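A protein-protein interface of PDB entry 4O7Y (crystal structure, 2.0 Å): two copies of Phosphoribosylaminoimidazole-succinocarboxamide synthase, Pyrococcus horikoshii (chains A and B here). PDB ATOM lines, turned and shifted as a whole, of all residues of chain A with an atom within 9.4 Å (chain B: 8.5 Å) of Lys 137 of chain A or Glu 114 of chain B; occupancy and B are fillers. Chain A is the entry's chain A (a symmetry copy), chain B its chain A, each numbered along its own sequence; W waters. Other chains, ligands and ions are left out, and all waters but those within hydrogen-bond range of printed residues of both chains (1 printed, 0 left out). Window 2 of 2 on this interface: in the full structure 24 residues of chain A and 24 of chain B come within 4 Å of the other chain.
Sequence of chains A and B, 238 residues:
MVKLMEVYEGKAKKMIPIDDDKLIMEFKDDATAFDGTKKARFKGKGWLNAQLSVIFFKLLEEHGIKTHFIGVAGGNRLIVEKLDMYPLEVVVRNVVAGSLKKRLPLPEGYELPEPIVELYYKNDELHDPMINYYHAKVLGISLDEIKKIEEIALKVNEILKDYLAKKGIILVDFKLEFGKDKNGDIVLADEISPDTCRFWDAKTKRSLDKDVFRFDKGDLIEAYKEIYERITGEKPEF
The backbone carbonyl oxygen (O) of Val 117 of chain B is in hydrogen-bond range of the side-chain amide nitrogen (ND2) of Asn 132 of chain A (2.8 Å).
The side-chain amide oxygen (OD1) of Asn 132 of chain A sits close to the backbone NH (N) of His 135 of chain A (3.2 Å). The backbone NH of Tyr 134 of chain A is in hydrogen-bond range of the side-chain amide oxygen of Asn 132 of chain A, at 2.8 Å. O of Ile 116 of chain B sits at hydrogen-bond distance from N of Arg 93 of chain B.
Among the printed residues, merely in contact across the chains: Tyr 134 of chain A with Pro 115 of chain B, Tyr 134 of chain A with Ile 116 of chain B, Tyr 134 of chain A with Val 117 of chain B, Tyr 134 of chain A with Leu 154 of chain B, His 135 of chain A with Leu 100 of chain B, His 135 of chain A with Ile 116 of chain B, Lys 137 of chain A with Glu 114 of chain B, Val 138 of chain A with Leu 104 of chain B, Val 138 of chain A with Ile 116 of chain B and Leu 139 of chain A with Leu 104 of chain B.
Of the printed residues of chain B, Lys 137 of chain A touches Glu 114 (3.5 Å). Printed residues of chain A within 4 Å of Glu 114 of chain B: Lys 137. No residue of chain B comes within 4 Å of Ala 136 of chain A. No residue of chain A comes within 4 Å of Pro 113 of chain B. Of chain A, only Tyr 134 comes within 4 Å of Pro 115 of chain B. Printed residues of chain B within 4 Å of Val 138 of chain A: Leu 104 (3.9 Å) and Ile 116 (3.9 Å). Printed residues of chain A within 4 Å of Leu 100 of chain B: His 135 (3.8 Å). Printed residues of chain B within 4 Å of His 135 of chain A: Leu 100 and Ile 116. Of the printed residues of chain A, Leu 104 of chain B touches Val 138 and Leu 139. Val 95 of chain B touches none of the printed residues of chain A.
Printed residues of chain A that touch a printed residue of chain B: Asn 132, Tyr 134, His 135, Lys 137, Val 138 and Leu 139. Hydrophobic or aromatic side chains of chain A that line the printed part of chain B: Tyr 134, His 135, Val 138 and Leu 139. Along chain A the printed residues that touch a printed residue of chain B span positions 132 to 139. Of the 18 printed residues of chain B, 7 touch a printed residue of chain A. Printed residues of chain B that touch a printed residue of chain A: Leu 100, Leu 104, Glu 114, Pro 115, Ile 116, Val 117 and Leu 154.
No position is printed for both chains. Of the 11 pairs that touch across the chains among the printed residues, none has its exchanged pair printed and touching as well.
Water W1 bridges O of Val 117 of chain B (3.0 Å) and ND2 of Asn 132 of chain A (3.2 Å).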
ATOM      1  N   LEU A  88     -10.978   1.100 -15.887  1.00  0.00           N
ATOM      2  CA  LEU A  88      -9.531   1.328 -15.871  1.00  0.00           C
ATOM      3  C   LEU A  88      -8.835   0.568 -16.952  1.00  0.00           C
ATOM      4  O   LEU A  88      -9.224  -0.553 -17.316  1.00  0.00           O
ATOM      5  CB  LEU A  88      -8.907   0.863 -14.540  1.00  0.00           C
ATOM      6  CG  LEU A  88      -9.407   1.558 -13.251  1.00  0.00           C
ATOM      7  CD1 LEU A  88      -8.870   0.819 -12.013  1.00  0.00           C
ATOM      8  CD2 LEU A  88      -9.030   3.029 -13.222  1.00  0.00           C
ATOM      9  N   LEU A 119      -2.266   4.090 -14.256  1.00  0.00           N
ATOM     10  CA  LEU A 119      -3.729   3.951 -14.318  1.00  0.00           C
ATOM     11  C   LEU A 119      -4.277   4.939 -15.321  1.00  0.00           C
ATOM     12  O   LEU A 119      -3.908   6.109 -15.254  1.00  0.00           O
ATOM     13  CB  LEU A 119      -4.361   4.247 -12.960  1.00  0.00           C
ATOM     14  CG  LEU A 119      -3.748   3.401 -11.826  1.00  0.00           C
ATOM     15  CD1 LEU A 119      -4.201   3.881 -10.451  1.00  0.00           C
ATOM     16  CD2 LEU A 119      -4.084   1.921 -12.053  1.00  0.00           C
ATOM     17  N   ILE A 131      -4.738   8.745 -14.654  1.00  0.00           N
ATOM     18  CA  ILE A 131      -5.247   9.211 -13.387  1.00  0.00           C
ATOM     19  C   ILE A 131      -4.361   8.723 -12.257  1.00  0.00           C
ATOM     20  O   ILE A 131      -3.496   7.867 -12.462  1.00  0.00           O
ATOM     21  CB  ILE A 131      -6.716   8.758 -13.129  1.00  0.00           C
ATOM     22  CG1 ILE A 131      -6.857   7.232 -13.274  1.00  0.00           C
ATOM     23  CG2 ILE A 131      -7.665   9.579 -14.021  1.00  0.00           C
ATOM     24  CD1 ILE A 131      -8.108   6.661 -12.594  1.00  0.00           C
ATOM     25  N   ASN A 132      -4.569   9.258 -11.061  1.00  0.00           N
ATOM     26  CA  ASN A 132      -3.877   8.678  -9.893  1.00  0.00           C
ATOM     27  C   ASN A 132      -4.912   8.072  -8.913  1.00  0.00           C
ATOM     28  O   ASN A 132      -6.129   7.991  -9.238  1.00  0.00           O
ATOM     29  CB  ASN A 132      -2.904   9.710  -9.257  1.00  0.00           C
ATOM     30  CG  ASN A 132      -3.611  10.927  -8.686  1.00  0.00           C
ATOM     31  OD1 ASN A 132      -4.707  10.826  -8.139  1.00  0.00           O
ATOM     32  ND2 ASN A 132      -2.960  12.087  -8.772  1.00  0.00           N
ATOM     33  N   TYR A 133      -4.440   7.625  -7.752  1.00  0.00           N
ATOM     34  CA  TYR A 133      -5.290   7.050  -6.714  1.00  0.00           C
ATOM     35  C   TYR A 133      -6.378   7.991  -6.228  1.00  0.00           C
ATOM     36  O   TYR A 133      -7.473   7.536  -5.849  1.00  0.00           O
ATOM     37  CB  TYR A 133      -4.455   6.563  -5.492  1.00  0.00           C
ATOM     38  CG  TYR A 133      -3.235   5.675  -5.808  1.00  0.00           C
ATOM     39  CD1 TYR A 133      -3.105   5.014  -7.040  1.00  0.00           C
ATOM     40  CD2 TYR A 133      -2.240   5.460  -4.847  1.00  0.00           C
ATOM     41  CE1 TYR A 133      -1.999   4.211  -7.328  1.00  0.00           C
ATOM     42  CE2 TYR A 133      -1.146   4.630  -5.119  1.00  0.00           C
ATOM     43  CZ  TYR A 133      -1.026   4.019  -6.353  1.00  0.00           C
ATOM     44  OH  TYR A 133       0.064   3.212  -6.611  1.00  0.00           O
ATOM     45  N   TYR A 134      -6.098   9.293  -6.188  1.00  0.00           N
ATOM     46  CA  TYR A 134      -7.117  10.249  -5.749  1.00  0.00           C
ATOM     47  C   TYR A 134      -8.233  10.370  -6.770  1.00  0.00           C
ATOM     48  O   TYR A 134      -9.401  10.455  -6.379  1.00  0.00           O
ATOM     49  CB  TYR A 134      -6.550  11.654  -5.486  1.00  0.00           C
ATOM     50  CG  TYR A 134      -5.511  11.694  -4.400  1.00  0.00           C
ATOM     51  CD1 TYR A 134      -5.870  12.049  -3.093  1.00  0.00           C
ATOM     52  CD2 TYR A 134      -4.176  11.367  -4.661  1.00  0.00           C
ATOM     53  CE1 TYR A 134      -4.950  12.068  -2.080  1.00  0.00           C
ATOM     54  CE2 TYR A 134      -3.236  11.399  -3.640  1.00  0.00           C
ATOM     55  CZ  TYR A 134      -3.648  11.754  -2.348  1.00  0.00           C
ATOM     56  OH  TYR A 134      -2.755  11.842  -1.320  1.00  0.00           O
ATOM     57  N   HIS A 135      -7.898  10.399  -8.068  1.00  0.00           N
ATOM     58  CA  HIS A 135      -8.957  10.501  -9.085  1.00  0.00           C
ATOM     59  C   HIS A 135      -9.765   9.227  -9.025  1.00  0.00           C
ATOM     60  O   HIS A 135     -10.987   9.265  -9.170  1.00  0.00           O
ATOM     61  CB  HIS A 135      -8.427  10.652 -10.519  1.00  0.00           C
ATOM     62  CG  HIS A 135      -7.383  11.746 -10.716  1.00  0.00           C
ATOM     63  ND1 HIS A 135      -7.692  13.054 -10.759  1.00  0.00           N
ATOM     64  CD2 HIS A 135      -6.034  11.665 -10.946  1.00  0.00           C
ATOM     65  CE1 HIS A 135      -6.579  13.769 -10.970  1.00  0.00           C
ATOM     66  NE2 HIS A 135      -5.564  12.911 -11.093  1.00  0.00           N
ATOM     67  N   ALA A 136      -9.094   8.084  -8.819  1.00  0.00           N
ATOM     68  CA  ALA A 136      -9.780   6.769  -8.745  1.00  0.00           C
ATOM     69  C   ALA A 136     -10.839   6.695  -7.611  1.00  0.00           C
ATOM     70  O   ALA A 136     -11.965   6.164  -7.798  1.00  0.00           O
ATOM     71  CB  ALA A 136      -8.763   5.662  -8.538  1.00  0.00           C
ATOM     72  N   LYS A 137     -10.450   7.209  -6.449  1.00  0.00           N
ATOM     73  CA  LYS A 137     -11.352   7.352  -5.323  1.00  0.00           C
ATOM     74  C   LYS A 137     -12.603   8.164  -5.698  1.00  0.00           C
ATOM     75  O   LYS A 137     -13.710   7.726  -5.408  1.00  0.00           O
ATOM     76  CB  LYS A 137     -10.614   7.931  -4.107  1.00  0.00           C
ATOM     77  CG  LYS A 137     -11.507   8.171  -2.897  1.00  0.00           C
ATOM     78  CD  LYS A 137     -12.020   6.878  -2.330  1.00  0.00           C
ATOM     79  CE  LYS A 137     -12.368   7.047  -0.858  1.00  0.00           C
ATOM     80  NZ  LYS A 137     -12.479   5.696  -0.233  1.00  0.00           N
ATOM     81  N   VAL A 138     -12.441   9.289  -6.394  1.00  0.00           N
ATOM     82  CA  VAL A 138     -13.621  10.078  -6.844  1.00  0.00           C
ATOM     83  C   VAL A 138     -14.477   9.283  -7.807  1.00  0.00           C
ATOM     84  O   VAL A 138     -15.707   9.446  -7.848  1.00  0.00           O
ATOM     85  CB  VAL A 138     -13.226  11.450  -7.471  1.00  0.00           C
ATOM     86  CG1 VAL A 138     -14.449  12.203  -8.014  1.00  0.00           C
ATOM     87  CG2 VAL A 138     -12.538  12.305  -6.427  1.00  0.00           C
ATOM     88  N   LEU A 139     -13.831   8.423  -8.583  1.00  0.00           N
ATOM     89  CA  LEU A 139     -14.532   7.513  -9.483  1.00  0.00           C
ATOM     90  C   LEU A 139     -15.180   6.311  -8.780  1.00  0.00           C
ATOM     91  O   LEU A 139     -15.809   5.502  -9.434  1.00  0.00           O
ATOM     92  CB  LEU A 139     -13.567   7.036 -10.584  1.00  0.00           C
ATOM     93  CG  LEU A 139     -13.213   8.108 -11.613  1.00  0.00           C
ATOM     94  CD1 LEU A 139     -12.088   7.566 -12.467  1.00  0.00           C
ATOM     95  CD2 LEU A 139     -14.408   8.541 -12.485  1.00  0.00           C
ATOM     96  N   GLY A 140     -15.016   6.194  -7.463  1.00  0.00           N
ATOM     97  CA  GLY A 140     -15.683   5.153  -6.661  1.00  0.00           C
ATOM     98  C   GLY A 140     -14.819   3.943  -6.367  1.00  0.00           C
ATOM     99  O   GLY A 140     -15.312   2.918  -5.888  1.00  0.00           O
ATOM    100  N   ILE A 141     -13.523   4.048  -6.658  1.00  0.00           N
ATOM    101  CA  ILE A 141     -12.569   2.943  -6.476  1.00  0.00           C
ATOM    102  C   ILE A 141     -11.684   3.236  -5.247  1.00  0.00           C
ATOM    103  O   ILE A 141     -10.902   4.202  -5.246  1.00  0.00           O
ATOM    104  CB  ILE A 141     -11.666   2.734  -7.739  1.00  0.00           C
ATOM    105  CG1 ILE A 141     -12.509   2.649  -9.027  1.00  0.00           C
ATOM    106  CG2 ILE A 141     -10.809   1.486  -7.574  1.00  0.00           C
ATOM    107  CD1 ILE A 141     -11.725   2.681 -10.329  1.00  0.00           C
ATOM    108  N   SER A 142     -11.783   2.382  -4.225  1.00  0.00           N
ATOM    109  CA  SER A 142     -11.121   2.593  -2.945  1.00  0.00           C
ATOM    110  C   SER A 142      -9.633   2.388  -3.066  1.00  0.00           C
ATOM    111  O   SER A 142      -9.164   1.730  -4.006  1.00  0.00           O
ATOM    112  CB  SER A 142     -11.681   1.656  -1.850  1.00  0.00           C
ATOM    113  OG  SER A 142     -11.263   0.310  -2.039  1.00  0.00           O
ATOM    114  N   LEU A 143      -8.891   2.970  -2.131  1.00  0.00           N
ATOM    115  CA  LEU A 143      -7.452   2.792  -2.097  1.00  0.00           C
ATOM    116  C   LEU A 143      -7.070   1.311  -1.969  1.00  0.00           C
ATOM    117  O   LEU A 143      -6.102   0.885  -2.606  1.00  0.00           O
ATOM    118  CB  LEU A 143      -6.810   3.657  -0.995  1.00  0.00           C
ATOM    119  CG  LEU A 143      -5.274   3.687  -1.000  1.00  0.00           C
ATOM    120  CD1 LEU A 143      -4.757   4.130  -2.362  1.00  0.00           C
ATOM    121  CD2 LEU A 143      -4.664   4.534   0.136  1.00  0.00           C
ATOM    122  N   ASP A 144      -7.818   0.540  -1.159  1.00  0.00           N
ATOM    123  CA  ASP A 144      -7.624  -0.926  -0.996  1.00  0.00           C
ATOM    124  C   ASP A 144      -7.748  -1.649  -2.342  1.00  0.00           C
ATOM    125  O   ASP A 144      -6.916  -2.496  -2.715  1.00  0.00           O
ATOM    126  CB  ASP A 144      -8.667  -1.489   0.003  1.00  0.00           C
ATOM    127  CG  ASP A 144      -8.637  -3.020   0.119  1.00  0.00           C
ATOM    128  OD1 ASP A 144      -7.566  -3.587   0.429  1.00  0.00           O
ATOM    129  OD2 ASP A 144      -9.699  -3.659  -0.072  1.00  0.00           O
ATOM    130  N   GLU A 145      -8.819  -1.336  -3.062  1.00  0.00           N
ATOM    131  CA  GLU A 145      -9.028  -1.902  -4.398  1.00  0.00           C
ATOM    132  C   GLU A 145      -7.886  -1.557  -5.365  1.00  0.00           C
ATOM    133  O   GLU A 145      -7.411  -2.449  -6.070  1.00  0.00           O
ATOM    134  CB  GLU A 145     -10.346  -1.453  -5.005  1.00  0.00           C
ATOM    135  CG  GLU A 145     -11.554  -2.076  -4.325  1.00  0.00           C
ATOM    136  CD  GLU A 145     -12.824  -1.425  -4.812  1.00  0.00           C
ATOM    137  OE1 GLU A 145     -13.110  -0.305  -4.373  1.00  0.00           O
ATOM    138  OE2 GLU A 145     -13.534  -2.019  -5.640  1.00  0.00           O
ATOM    139  N   ILE A 146      -7.464  -0.282  -5.388  1.00  0.00           N
ATOM    140  CA  ILE A 146      -6.346   0.158  -6.256  1.00  0.00           C
ATOM    141  C   ILE A 146      -5.057  -0.571  -5.866  1.00  0.00           C
ATOM    142  O   ILE A 146      -4.358  -1.094  -6.717  1.00  0.00           O
ATOM    143  CB  ILE A 146      -6.136   1.689  -6.180  1.00  0.00           C
ATOM    144  CG1 ILE A 146      -7.156   2.444  -7.049  1.00  0.00           C
ATOM    145  CG2 ILE A 146      -4.710   2.075  -6.544  1.00  0.00           C
ATOM    146  CD1 ILE A 146      -7.160   2.086  -8.522  1.00  0.00           C
ATOM    147  N   VAL B  92      -3.091  20.509  -5.269  1.00  0.00           N
ATOM    148  CA  VAL B  92      -4.168  20.040  -4.384  1.00  0.00           C
ATOM    149  C   VAL B  92      -5.455  20.690  -4.890  1.00  0.00           C
ATOM    150  O   VAL B  92      -5.466  21.883  -5.146  1.00  0.00           O
ATOM    151  CB  VAL B  92      -3.927  20.451  -2.914  1.00  0.00           C
ATOM    152  CG1 VAL B  92      -5.001  19.872  -2.006  1.00  0.00           C
ATOM    153  CG2 VAL B  92      -2.557  20.005  -2.454  1.00  0.00           C
ATOM    154  N   ARG B  93      -6.519  19.895  -5.041  1.00  0.00           N
ATOM    155  CA  ARG B  93      -7.774  20.378  -5.621  1.00  0.00           C
ATOM    156  C   ARG B  93      -8.972  20.033  -4.711  1.00  0.00           C
ATOM    157  O   ARG B  93      -9.130  18.890  -4.290  1.00  0.00           O
ATOM    158  CB  ARG B  93      -7.943  19.799  -7.035  1.00  0.00           C
ATOM    159  CG  ARG B  93      -6.609  19.577  -7.760  1.00  0.00           C
ATOM    160  CD  ARG B  93      -6.749  19.136  -9.214  1.00  0.00           C
ATOM    161  NE  ARG B  93      -7.225  20.237 -10.031  1.00  0.00           N
ATOM    162  CZ  ARG B  93      -6.577  20.813 -11.043  1.00  0.00           C
ATOM    163  NH1 ARG B  93      -5.381  20.386 -11.463  1.00  0.00           N
ATOM    164  NH2 ARG B  93      -7.173  21.823 -11.669  1.00  0.00           N
ATOM    165  N   ASN B  94      -9.778  21.044  -4.381  1.00  0.00           N
ATOM    166  CA  ASN B  94     -11.003  20.888  -3.570  1.00  0.00           C
ATOM    167  C   ASN B  94     -12.273  20.971  -4.407  1.00  0.00           C
ATOM    168  O   ASN B  94     -13.275  20.298  -4.106  1.00  0.00           O
ATOM    169  CB  ASN B  94     -11.048  21.936  -2.466  1.00  0.00           C
ATOM    170  CG  ASN B  94      -9.825  21.862  -1.565  1.00  0.00           C
ATOM    171  OD1 ASN B  94      -9.535  20.799  -0.977  1.00  0.00           O
ATOM    172  ND2 ASN B  94      -9.076  22.956  -1.486  1.00  0.00           N
ATOM    173  N   VAL B  95     -12.195  21.760  -5.477  1.00  0.00           N
ATOM    174  CA  VAL B  95     -13.331  22.071  -6.336  1.00  0.00           C
ATOM    175  C   VAL B  95     -12.871  21.893  -7.789  1.00  0.00           C
ATOM    176  O   VAL B  95     -11.746  22.286  -8.111  1.00  0.00           O
ATOM    177  CB  VAL B  95     -13.761  23.527  -6.075  1.00  0.00           C
ATOM    178  CG1 VAL B  95     -14.777  24.002  -7.108  1.00  0.00           C
ATOM    179  CG2 VAL B  95     -14.309  23.662  -4.648  1.00  0.00           C
ATOM    180  N   LEU B 100      -8.487  19.662 -14.462  1.00  0.00           N
ATOM    181  CA  LEU B 100      -9.261  18.548 -13.898  1.00  0.00           C
ATOM    182  C   LEU B 100     -10.534  18.222 -14.720  1.00  0.00           C
ATOM    183  O   LEU B 100     -10.968  17.083 -14.767  1.00  0.00           O
ATOM    184  CB  LEU B 100      -9.600  18.796 -12.411  1.00  0.00           C
ATOM    185  CG  LEU B 100     -10.175  17.559 -11.702  1.00  0.00           C
ATOM    186  CD1 LEU B 100      -9.268  16.332 -11.860  1.00  0.00           C
ATOM    187  CD2 LEU B 100     -10.414  17.884 -10.226  1.00  0.00           C
ATOM    188  N   LEU B 104     -11.544  14.251 -15.377  1.00  0.00           N
ATOM    189  CA  LEU B 104     -12.778  13.693 -14.792  1.00  0.00           C
ATOM    190  C   LEU B 104     -14.020  14.393 -15.422  1.00  0.00           C
ATOM    191  O   LEU B 104     -14.023  15.621 -15.604  1.00  0.00           O
ATOM    192  CB  LEU B 104     -12.800  13.839 -13.251  1.00  0.00           C
ATOM    193  CG  LEU B 104     -11.781  13.003 -12.422  1.00  0.00           C
ATOM    194  CD1 LEU B 104     -11.977  13.150 -10.914  1.00  0.00           C
ATOM    195  CD2 LEU B 104     -11.839  11.518 -12.797  1.00  0.00           C
ATOM    196  N   TYR B 110     -17.845  21.690  -9.349  1.00  0.00           N
ATOM    197  CA  TYR B 110     -18.148  20.480  -8.594  1.00  0.00           C
ATOM    198  C   TYR B 110     -17.306  20.417  -7.314  1.00  0.00           C
ATOM    199  O   TYR B 110     -16.073  20.605  -7.327  1.00  0.00           O
ATOM    200  CB  TYR B 110     -17.948  19.260  -9.478  1.00  0.00           C
ATOM    201  CG  TYR B 110     -18.369  17.898  -8.926  1.00  0.00           C
ATOM    202  CD1 TYR B 110     -19.552  17.270  -9.377  1.00  0.00           C
ATOM    203  CD2 TYR B 110     -17.549  17.195  -8.021  1.00  0.00           C
ATOM    204  CE1 TYR B 110     -19.907  16.006  -8.918  1.00  0.00           C
ATOM    205  CE2 TYR B 110     -17.898  15.912  -7.570  1.00  0.00           C
ATOM    206  CZ  TYR B 110     -19.073  15.330  -8.022  1.00  0.00           C
ATOM    207  OH  TYR B 110     -19.413  14.075  -7.569  1.00  0.00           O
ATOM    208  N   GLU B 111     -17.984  20.206  -6.190  1.00  0.00           N
ATOM    209  CA  GLU B 111     -17.290  20.088  -4.927  1.00  0.00           C
ATOM    210  C   GLU B 111     -16.848  18.647  -4.734  1.00  0.00           C
ATOM    211  O   GLU B 111     -17.666  17.714  -4.732  1.00  0.00           O
ATOM    212  CB  GLU B 111     -18.170  20.550  -3.778  1.00  0.00           C
ATOM    213  CG  GLU B 111     -17.407  20.734  -2.487  1.00  0.00           C
ATOM    214  CD  GLU B 111     -18.345  20.805  -1.309  1.00  0.00           C
ATOM    215  OE1 GLU B 111     -18.497  21.904  -0.751  1.00  0.00           O
ATOM    216  OE2 GLU B 111     -18.935  19.767  -0.970  1.00  0.00           O
ATOM    217  N   LEU B 112     -15.540  18.458  -4.616  1.00  0.00           N
ATOM    218  CA  LEU B 112     -15.029  17.102  -4.530  1.00  0.00           C
ATOM    219  C   LEU B 112     -15.350  16.505  -3.158  1.00  0.00           C
ATOM    220  O   LEU B 112     -15.312  17.238  -2.158  1.00  0.00           O
ATOM    221  CB  LEU B 112     -13.509  17.055  -4.806  1.00  0.00           C
ATOM    222  CG  LEU B 112     -13.116  17.419  -6.247  1.00  0.00           C
ATOM    223  CD1 LEU B 112     -11.618  17.721  -6.383  1.00  0.00           C
ATOM    224  CD2 LEU B 112     -13.520  16.312  -7.220  1.00  0.00           C
ATOM    225  N   PRO B 113     -15.631  15.184  -3.105  1.00  0.00           N
ATOM    226  CA  PRO B 113     -15.913  14.516  -1.824  1.00  0.00           C
ATOM    227  C   PRO B 113     -14.684  14.584  -0.894  1.00  0.00           C
ATOM    228  O   PRO B 113     -14.840  14.706   0.316  1.00  0.00           O
ATOM    229  CB  PRO B 113     -16.253  13.069  -2.233  1.00  0.00           C
ATOM    230  CG  PRO B 113     -15.601  12.865  -3.585  1.00  0.00           C
ATOM    231  CD  PRO B 113     -15.589  14.231  -4.241  1.00  0.00           C
ATOM    232  N   GLU B 114     -13.474  14.532  -1.469  1.00  0.00           N
ATOM    233  CA  GLU B 114     -12.238  14.697  -0.689  1.00  0.00           C
ATOM    234  C   GLU B 114     -11.163  15.346  -1.577  1.00  0.00           C
ATOM    235  O   GLU B 114     -11.274  15.316  -2.807  1.00  0.00           O
ATOM    236  CB  GLU B 114     -11.764  13.358  -0.095  1.00  0.00           C
ATOM    237  CG  GLU B 114     -11.232  12.336  -1.097  1.00  0.00           C
ATOM    238  CD  GLU B 114     -10.723  11.054  -0.441  1.00  0.00           C
ATOM    239  OE1 GLU B 114      -9.494  10.825  -0.450  1.00  0.00           O
ATOM    240  OE2 GLU B 114     -11.547  10.271   0.080  1.00  0.00           O
ATOM    241  N   PRO B 115     -10.115  15.948  -0.962  1.00  0.00           N
ATOM    242  CA  PRO B 115      -9.141  16.608  -1.856  1.00  0.00           C
ATOM    243  C   PRO B 115      -8.397  15.631  -2.793  1.00  0.00           C
ATOM    244  O   PRO B 115      -8.095  14.511  -2.398  1.00  0.00           O
ATOM    245  CB  PRO B 115      -8.157  17.277  -0.885  1.00  0.00           C
ATOM    246  CG  PRO B 115      -8.867  17.343   0.428  1.00  0.00           C
ATOM    247  CD  PRO B 115      -9.787  16.156   0.469  1.00  0.00           C
ATOM    248  N   ILE B 116      -8.174  16.041  -4.044  1.00  0.00           N
ATOM    249  CA  ILE B 116      -7.285  15.345  -4.986  1.00  0.00           C
ATOM    250  C   ILE B 116      -5.856  15.931  -4.921  1.00  0.00           C
ATOM    251  O   ILE B 116      -5.694  17.139  -4.899  1.00  0.00           O
ATOM    252  CB  ILE B 116      -7.856  15.503  -6.415  1.00  0.00           C
ATOM    253  CG1 ILE B 116      -9.185  14.729  -6.489  1.00  0.00           C
ATOM    254  CG2 ILE B 116      -6.841  15.055  -7.467  1.00  0.00           C
ATOM    255  CD1 ILE B 116      -9.801  14.605  -7.876  1.00  0.00           C
ATOM    256  N   VAL B 117      -4.822  15.097  -4.874  1.00  0.00           N
ATOM    257  CA  VAL B 117      -3.436  15.611  -4.960  1.00  0.00           C
ATOM    258  C   VAL B 117      -2.914  15.107  -6.305  1.00  0.00           C
ATOM    259  O   VAL B 117      -3.076  13.906  -6.626  1.00  0.00           O
ATOM    260  CB  VAL B 117      -2.524  15.065  -3.842  1.00  0.00           C
ATOM    261  CG1 VAL B 117      -1.131  15.673  -3.930  1.00  0.00           C
ATOM    262  CG2 VAL B 117      -3.141  15.306  -2.454  1.00  0.00           C
ATOM    263  N   LEU B 154      -1.613  18.268   1.895  1.00  0.00           N
ATOM    264  CA  LEU B 154      -2.972  18.101   2.444  1.00  0.00           C
ATOM    265  C   LEU B 154      -3.179  18.860   3.743  1.00  0.00           C
ATOM    266  O   LEU B 154      -4.275  19.385   3.985  1.00  0.00           O
ATOM    267  CB  LEU B 154      -3.285  16.603   2.633  1.00  0.00           C
ATOM    268  CG  LEU B 154      -3.486  15.846   1.339  1.00  0.00           C
ATOM    269  CD1 LEU B 154      -3.533  14.355   1.670  1.00  0.00           C
ATOM    270  CD2 LEU B 154      -4.760  16.312   0.638  1.00  0.00           C
ATOM    271  N   ASN B 157      -3.385  22.473   2.665  1.00  0.00           N
ATOM    272  CA  ASN B 157      -4.761  22.620   2.187  1.00  0.00           C
ATOM    273  C   ASN B 157      -5.756  22.926   3.308  1.00  0.00           C
ATOM    274  O   ASN B 157      -6.483  23.904   3.224  1.00  0.00           O
ATOM    275  CB  ASN B 157      -5.187  21.340   1.502  1.00  0.00           C
ATOM    276  CG  ASN B 157      -6.511  21.478   0.764  1.00  0.00           C
ATOM    277  OD1 ASN B 157      -6.814  22.519   0.137  1.00  0.00           O
ATOM    278  ND2 ASN B 157      -7.308  20.425   0.824  1.00  0.00           N
ATOM    279  N   GLU B 158      -5.800  22.056   4.330  1.00  0.00           N
ATOM    280  CA  GLU B 158      -6.666  22.259   5.492  1.00  0.00           C
ATOM    281  C   GLU B 158      -6.497  23.653   6.092  1.00  0.00           C
ATOM    282  O   GLU B 158      -7.475  24.368   6.246  1.00  0.00           O
ATOM    283  CB  GLU B 158      -6.469  21.160   6.564  1.00  0.00           C
ATOM    284  CG  GLU B 158      -6.973  19.787   6.142  1.00  0.00           C
ATOM    285  CD  GLU B 158      -8.398  19.797   5.573  1.00  0.00           C
ATOM    286  OE1 GLU B 158      -8.590  19.504   4.364  1.00  0.00           O
ATOM    287  OE2 GLU B 158      -9.342  20.093   6.333  1.00  0.00           O
ATOM    288  N   LYS B 161      -7.523  26.586   3.356  1.00  0.00           N
ATOM    289  CA  LYS B 161      -8.946  26.576   3.056  1.00  0.00           C
ATOM    290  C   LYS B 161      -9.803  27.047   4.250  1.00  0.00           C
ATOM    291  O   LYS B 161     -10.710  27.851   4.059  1.00  0.00           O
ATOM    292  CB  LYS B 161      -9.402  25.207   2.501  1.00  0.00           C
ATOM    293  CG  LYS B 161      -9.578  24.102   3.524  1.00  0.00           C
ATOM    294  CD  LYS B 161      -9.691  22.715   2.886  1.00  0.00           C
ATOM    295  CE  LYS B 161     -10.865  22.636   1.933  1.00  0.00           C
ATOM    296  NZ  LYS B 161     -12.104  22.269   2.677  1.00  0.00           N
HETATM  297  O   HOH W   1      -1.002  11.781  -6.246  1.00  0.00           O
